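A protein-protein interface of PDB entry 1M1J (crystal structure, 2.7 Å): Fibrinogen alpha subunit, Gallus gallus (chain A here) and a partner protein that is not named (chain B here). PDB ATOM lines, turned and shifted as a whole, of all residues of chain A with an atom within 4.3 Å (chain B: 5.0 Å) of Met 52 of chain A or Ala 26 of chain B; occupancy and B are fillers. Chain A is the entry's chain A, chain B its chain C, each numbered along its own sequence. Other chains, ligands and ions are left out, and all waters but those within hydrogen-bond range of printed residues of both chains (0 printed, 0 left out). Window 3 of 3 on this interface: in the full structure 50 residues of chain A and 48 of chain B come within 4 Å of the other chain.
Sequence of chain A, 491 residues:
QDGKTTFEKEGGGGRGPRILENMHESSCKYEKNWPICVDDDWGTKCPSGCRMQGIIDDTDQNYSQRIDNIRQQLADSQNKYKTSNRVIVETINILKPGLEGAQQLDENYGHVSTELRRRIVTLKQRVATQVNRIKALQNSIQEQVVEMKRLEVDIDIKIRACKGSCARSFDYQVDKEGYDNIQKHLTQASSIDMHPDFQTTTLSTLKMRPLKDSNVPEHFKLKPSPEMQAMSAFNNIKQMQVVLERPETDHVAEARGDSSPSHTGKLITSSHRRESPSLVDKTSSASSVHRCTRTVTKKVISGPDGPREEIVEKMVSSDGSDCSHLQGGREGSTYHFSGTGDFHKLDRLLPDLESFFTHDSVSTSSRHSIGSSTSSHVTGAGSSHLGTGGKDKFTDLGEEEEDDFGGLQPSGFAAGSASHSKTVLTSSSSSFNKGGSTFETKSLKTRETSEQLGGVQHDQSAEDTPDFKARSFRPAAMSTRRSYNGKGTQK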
ATOM      1  N   PRO A  47       2.445  -7.505   0.714  1.00  0.00           N
ATOM      2  CA  PRO A  47       1.327  -6.558   0.685  1.00  0.00           C
ATOM      3  C   PRO A  47       1.734  -5.120   0.392  1.00  0.00           C
ATOM      4  O   PRO A  47       2.867  -4.714   0.663  1.00  0.00           O
ATOM      5  CB  PRO A  47       0.721  -6.705   2.078  1.00  0.00           C
ATOM      6  CG  PRO A  47       1.008  -8.127   2.417  1.00  0.00           C
ATOM      7  CD  PRO A  47       2.438  -8.266   1.977  1.00  0.00           C
ATOM      8  N   SER A  48       0.793  -4.359  -0.160  1.00  0.00           N
ATOM      9  CA  SER A  48       1.016  -2.955  -0.482  1.00  0.00           C
ATOM     10  C   SER A  48       1.606  -2.215   0.722  1.00  0.00           C
ATOM     11  O   SER A  48       1.694  -2.765   1.821  1.00  0.00           O
ATOM     12  CB  SER A  48      -0.312  -2.306  -0.889  1.00  0.00           C
ATOM     13  OG  SER A  48      -0.170  -0.908  -1.074  1.00  0.00           O
ATOM     14  N   GLY A  49       2.019  -0.971   0.516  1.00  0.00           N
ATOM     15  CA  GLY A  49       2.574  -0.204   1.615  1.00  0.00           C
ATOM     16  C   GLY A  49       1.458   0.522   2.338  1.00  0.00           C
ATOM     17  O   GLY A  49       1.567   0.839   3.522  1.00  0.00           O
ATOM     18  N   CYS A  50       0.371   0.773   1.618  1.00  0.00           N
ATOM     19  CA  CYS A  50      -0.778   1.473   2.175  1.00  0.00           C
ATOM     20  C   CYS A  50      -1.803   0.518   2.779  1.00  0.00           C
ATOM     21  O   CYS A  50      -2.556   0.898   3.674  1.00  0.00           O
ATOM     22  CB  CYS A  50      -1.432   2.341   1.096  1.00  0.00           C
ATOM     23  SG  CYS A  50      -0.634   2.156  -0.524  1.00  0.00           S
ATOM     24  N   ARG A  51      -1.837  -0.720   2.293  1.00  0.00           N
ATOM     25  CA  ARG A  51      -2.773  -1.699   2.832  1.00  0.00           C
ATOM     26  C   ARG A  51      -2.365  -2.063   4.257  1.00  0.00           C
ATOM     27  O   ARG A  51      -3.199  -2.486   5.058  1.00  0.00           O
ATOM     28  CB  ARG A  51      -2.813  -2.961   1.963  1.00  0.00           C
ATOM     29  CG  ARG A  51      -3.713  -4.067   2.512  1.00  0.00           C
ATOM     30  CD  ARG A  51      -5.110  -3.543   2.798  1.00  0.00           C
ATOM     31  NE  ARG A  51      -5.753  -3.017   1.599  1.00  0.00           N
ATOM     32  CZ  ARG A  51      -6.184  -3.769   0.591  1.00  0.00           C
ATOM     33  NH1 ARG A  51      -6.042  -5.087   0.639  1.00  0.00           N
ATOM     34  NH2 ARG A  51      -6.760  -3.204  -0.464  1.00  0.00           N
ATOM     35  N   MET A  52      -1.078  -1.904   4.566  1.00  0.00           N
ATOM     36  CA  MET A  52      -0.581  -2.198   5.906  1.00  0.00           C
ATOM     37  C   MET A  52      -0.880  -1.038   6.850  1.00  0.00           C
ATOM     38  O   MET A  52      -1.409  -1.242   7.940  1.00  0.00           O
ATOM     39  CB  MET A  52       0.928  -2.455   5.907  1.00  0.00           C
ATOM     40  CG  MET A  52       1.375  -3.820   5.430  1.00  0.00           C
ATOM     41  SD  MET A  52       0.665  -5.265   6.222  1.00  0.00           S
ATOM     42  CE  MET A  52      -0.925  -5.352   5.360  1.00  0.00           C
ATOM     43  N   GLN A  53      -0.534   0.178   6.436  1.00  0.00           N
ATOM     44  CA  GLN A  53      -0.784   1.353   7.264  1.00  0.00           C
ATOM     45  C   GLN A  53      -2.281   1.626   7.263  1.00  0.00           C
ATOM     46  O   GLN A  53      -2.747   2.584   7.876  1.00  0.00           O
ATOM     47  CB  GLN A  53      -0.046   2.575   6.712  1.00  0.00           C
ATOM     48  CG  GLN A  53      -0.056   3.797   7.629  1.00  0.00           C
ATOM     49  CD  GLN A  53       1.101   3.803   8.624  1.00  0.00           C
ATOM     50  OE1 GLN A  53       1.244   2.889   9.439  1.00  0.00           O
ATOM     51  NE2 GLN A  53       1.933   4.839   8.559  1.00  0.00           N
ATOM     52  N   GLY A  54      -3.026   0.777   6.557  1.00  0.00           N
ATOM     53  CA  GLY A  54      -4.469   0.927   6.482  1.00  0.00           C
ATOM     54  C   GLY A  54      -5.169   0.023   7.474  1.00  0.00           C
ATOM     55  O   GLY A  54      -6.290   0.297   7.899  1.00  0.00           O
ATOM     56  N   ILE A  55      -4.503  -1.066   7.843  1.00  0.00           N
ATOM     57  CA  ILE A  55      -5.051  -2.013   8.801  1.00  0.00           C
ATOM     58  C   ILE A  55      -4.484  -1.746  10.193  1.00  0.00           C
ATOM     59  O   ILE A  55      -5.224  -1.721  11.176  1.00  0.00           O
ATOM     60  CB  ILE A  55      -4.745  -3.466   8.383  1.00  0.00           C
ATOM     61  CG1 ILE A  55      -5.552  -3.812   7.130  1.00  0.00           C
ATOM     62  CG2 ILE A  55      -5.072  -4.425   9.523  1.00  0.00           C
ATOM     63  CD1 ILE A  55      -5.419  -5.250   6.686  1.00  0.00           C
ATOM     64  N   ILE A  56      -3.172  -1.540  10.275  1.00  0.00           N
ATOM     65  CA  ILE A  56      -2.531  -1.259  11.553  1.00  0.00           C
ATOM     66  C   ILE A  56      -3.212  -0.057  12.200  1.00  0.00           C
ATOM     67  O   ILE A  56      -2.976   0.251  13.372  1.00  0.00           O
ATOM     68  CB  ILE A  56      -1.024  -0.981  11.372  1.00  0.00           C
ATOM     69  CG1 ILE A  56      -0.311  -2.277  10.975  1.00  0.00           C
ATOM     70  CG2 ILE A  56      -0.424  -0.432  12.659  1.00  0.00           C
ATOM     71  CD1 ILE A  56       1.192  -2.133  10.821  1.00  0.00           C
ATOM     72  N   THR B  22       7.205  -5.562   3.862  1.00  0.00           N
ATOM     73  CA  THR B  22       5.818  -5.502   4.323  1.00  0.00           C
ATOM     74  C   THR B  22       5.292  -6.909   4.604  1.00  0.00           C
ATOM     75  O   THR B  22       4.090  -7.129   4.762  1.00  0.00           O
ATOM     76  CB  THR B  22       4.892  -4.825   3.296  1.00  0.00           C
ATOM     77  OG1 THR B  22       4.749  -5.662   2.144  1.00  0.00           O
ATOM     78  CG2 THR B  22       5.450  -3.478   2.889  1.00  0.00           C
ATOM     79  N   CYS B  23       6.219  -7.855   4.650  1.00  0.00           N
ATOM     80  CA  CYS B  23       5.936  -9.252   4.933  1.00  0.00           C
ATOM     81  C   CYS B  23       6.264  -9.415   6.411  1.00  0.00           C
ATOM     82  O   CYS B  23       5.492  -9.987   7.182  1.00  0.00           O
ATOM     83  CB  CYS B  23       6.874 -10.146   4.122  1.00  0.00           C
ATOM     84  SG  CYS B  23       6.342 -10.692   2.470  1.00  0.00           S
ATOM     85  N   GLY B  24       7.438  -8.906   6.781  1.00  0.00           N
ATOM     86  CA  GLY B  24       7.895  -8.970   8.155  1.00  0.00           C
ATOM     87  C   GLY B  24       7.084  -8.020   9.012  1.00  0.00           C
ATOM     88  O   GLY B  24       7.143  -8.063  10.242  1.00  0.00           O
ATOM     89  N   ILE B  25       6.331  -7.148   8.347  1.00  0.00           N
ATOM     90  CA  ILE B  25       5.473  -6.189   9.026  1.00  0.00           C
ATOM     91  C   ILE B  25       4.118  -6.850   9.246  1.00  0.00           C
ATOM     92  O   ILE B  25       3.533  -6.730  10.319  1.00  0.00           O
ATOM     93  CB  ILE B  25       5.284  -4.900   8.190  1.00  0.00           C
ATOM     94  CG1 ILE B  25       6.557  -4.052   8.245  1.00  0.00           C
ATOM     95  CG2 ILE B  25       4.090  -4.107   8.701  1.00  0.00           C
ATOM     96  CD1 ILE B  25       6.939  -3.603   9.638  1.00  0.00           C
ATOM     97  N   ALA B  26       3.624  -7.548   8.227  1.00  0.00           N
ATOM     98  CA  ALA B  26       2.346  -8.242   8.343  1.00  0.00           C
ATOM     99  C   ALA B  26       2.552  -9.478   9.222  1.00  0.00           C
ATOM    100  O   ALA B  26       1.600 -10.069   9.730  1.00  0.00           O
ATOM    101  CB  ALA B  26       1.841  -8.645   6.965  1.00  0.00           C
ATOM    102  N   ASP B  27       3.817  -9.846   9.395  1.00  0.00           N
ATOM    103  CA  ASP B  27       4.210 -10.996  10.203  1.00  0.00           C
ATOM    104  C   ASP B  27       4.161 -10.665  11.693  1.00  0.00           C
ATOM    105  O   ASP B  27       3.475 -11.332  12.467  1.00  0.00           O
ATOM    106  CB  ASP B  27       5.626 -11.435   9.806  1.00  0.00           C
ATOM    107  CG  ASP B  27       6.238 -12.421  10.788  1.00  0.00           C
ATOM    108  OD1 ASP B  27       6.492 -12.034  11.951  1.00  0.00           O
ATOM    109  OD2 ASP B  27       6.471 -13.584  10.391  1.00  0.00           O
ATOM    110  N   PHE B  28       4.904  -9.636  12.088  1.00  0.00           N
ATOM    111  CA  PHE B  28       4.954  -9.204  13.478  1.00  0.00           C
ATOM    112  C   PHE B  28       3.587  -8.675  13.878  1.00  0.00           C
ATOM    113  O   PHE B  28       3.263  -8.602  15.059  1.00  0.00           O
ATOM    114  CB  PHE B  28       5.988  -8.092  13.637  1.00  0.00           C
ATOM    115  CG  PHE B  28       6.190  -7.639  15.058  1.00  0.00           C
ATOM    116  CD1 PHE B  28       6.966  -8.388  15.940  1.00  0.00           C
ATOM    117  CD2 PHE B  28       5.636  -6.442  15.505  1.00  0.00           C
ATOM    118  CE1 PHE B  28       7.197  -7.951  17.248  1.00  0.00           C
ATOM    119  CE2 PHE B  28       5.857  -5.994  16.808  1.00  0.00           C
ATOM    120  CZ  PHE B  28       6.642  -6.751  17.683  1.00  0.00           C
ATOM    121  N   PHE B  29       2.787  -8.312  12.880  1.00  0.00           N
ATOM    122  CA  PHE B  29       1.457  -7.771  13.115  1.00  0.00           C
ATOM    123  C   PHE B  29       0.384  -8.798  13.463  1.00  0.00           C
ATOM    124  O   PHE B  29      -0.663  -8.439  13.996  1.00  0.00           O
ATOM    125  CB  PHE B  29       0.997  -6.970  11.908  1.00  0.00           C
ATOM    126  CG  PHE B  29      -0.355  -6.364  12.074  1.00  0.00           C
ATOM    127  CD1 PHE B  29      -0.596  -5.443  13.088  1.00  0.00           C
ATOM    128  CD2 PHE B  29      -1.393  -6.709  11.215  1.00  0.00           C
ATOM    129  CE1 PHE B  29      -1.850  -4.872  13.244  1.00  0.00           C
ATOM    130  CE2 PHE B  29      -2.656  -6.144  11.360  1.00  0.00           C
ATOM    131  CZ  PHE B  29      -2.886  -5.223  12.376  1.00  0.00           C
ATOM    132  N   ASN B  30       0.612 -10.064  13.140  1.00  0.00           N
ATOM    133  CA  ASN B  30      -0.367 -11.084  13.492  1.00  0.00           C
ATOM    134  C   ASN B  30      -0.025 -11.586  14.884  1.00  0.00           C
ATOM    135  O   ASN B  30      -0.903 -11.981  15.641  1.00  0.00           O
ATOM    136  CB  ASN B  30      -0.359 -12.246  12.497  1.00  0.00           C
ATOM    137  CG  ASN B  30      -1.430 -12.104  11.430  1.00  0.00           C
ATOM    138  OD1 ASN B  30      -1.754 -13.062  10.733  1.00  0.00           O
ATOM    139  ND2 ASN B  30      -1.984 -10.901  11.298  1.00  0.00           N
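Gly 54 of chain A touches none of the printed residues of chain B.
Of the printed residues of chain B, Ile 55 of chain A touches Phe 29 (3.5 Å).
Of the printed residues of chain B, Ile 56 of chain A touches Phe 29.
Ala 26 of chain B touches one residue of chain A.
Printed residues of chain A within 4 Å of Phe 29 of chain B: Ile 55 and Ile 56.
The nearest residue of chain B that does not touch Met 52 of chain A is Thr 22 of chain B (4.2 Å).
The nearest printed residue of chain A that does not touch Ala 26 of chain B is Pro 47 of chain A (4.7 Å).
The nearest printed residue of chain A that does not touch Thr 22 of chain B is Met 52 of chain A (4.2 Å).
Hydrophobic or aromatic side chains of chain A within 4 Å of the printed part of chain B: Pro 47, Met 52, Ile 55 and Ile 56.
Hydrophobic or aromatic side chains of chain B within 4 Å of the printed part of chain A: Ala 26 and Phe 29.
Among the printed residues, 5 pairs touch across the chains.
The side-chain hydroxyl of Thr 22 of chain B is in hydrogen-bond range of the backbone carbonyl oxygen of Pro 47 of chain A (2.6 Å).
OG of Ser 48 of chain A sits at hydrogen-bond distance from SG of Cys 50 of chain A (3.1 Å).
CG2 of Thr 22 of chain B touches O of Ser 48 of chain A, 3.97 Å away.
Ala 26 of chain B touches Met 52 of chain A.
Phe 29 of chain B touches Ile 55 of chain A.
Ile 56 of chain A touches Phe 29 of chain B.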
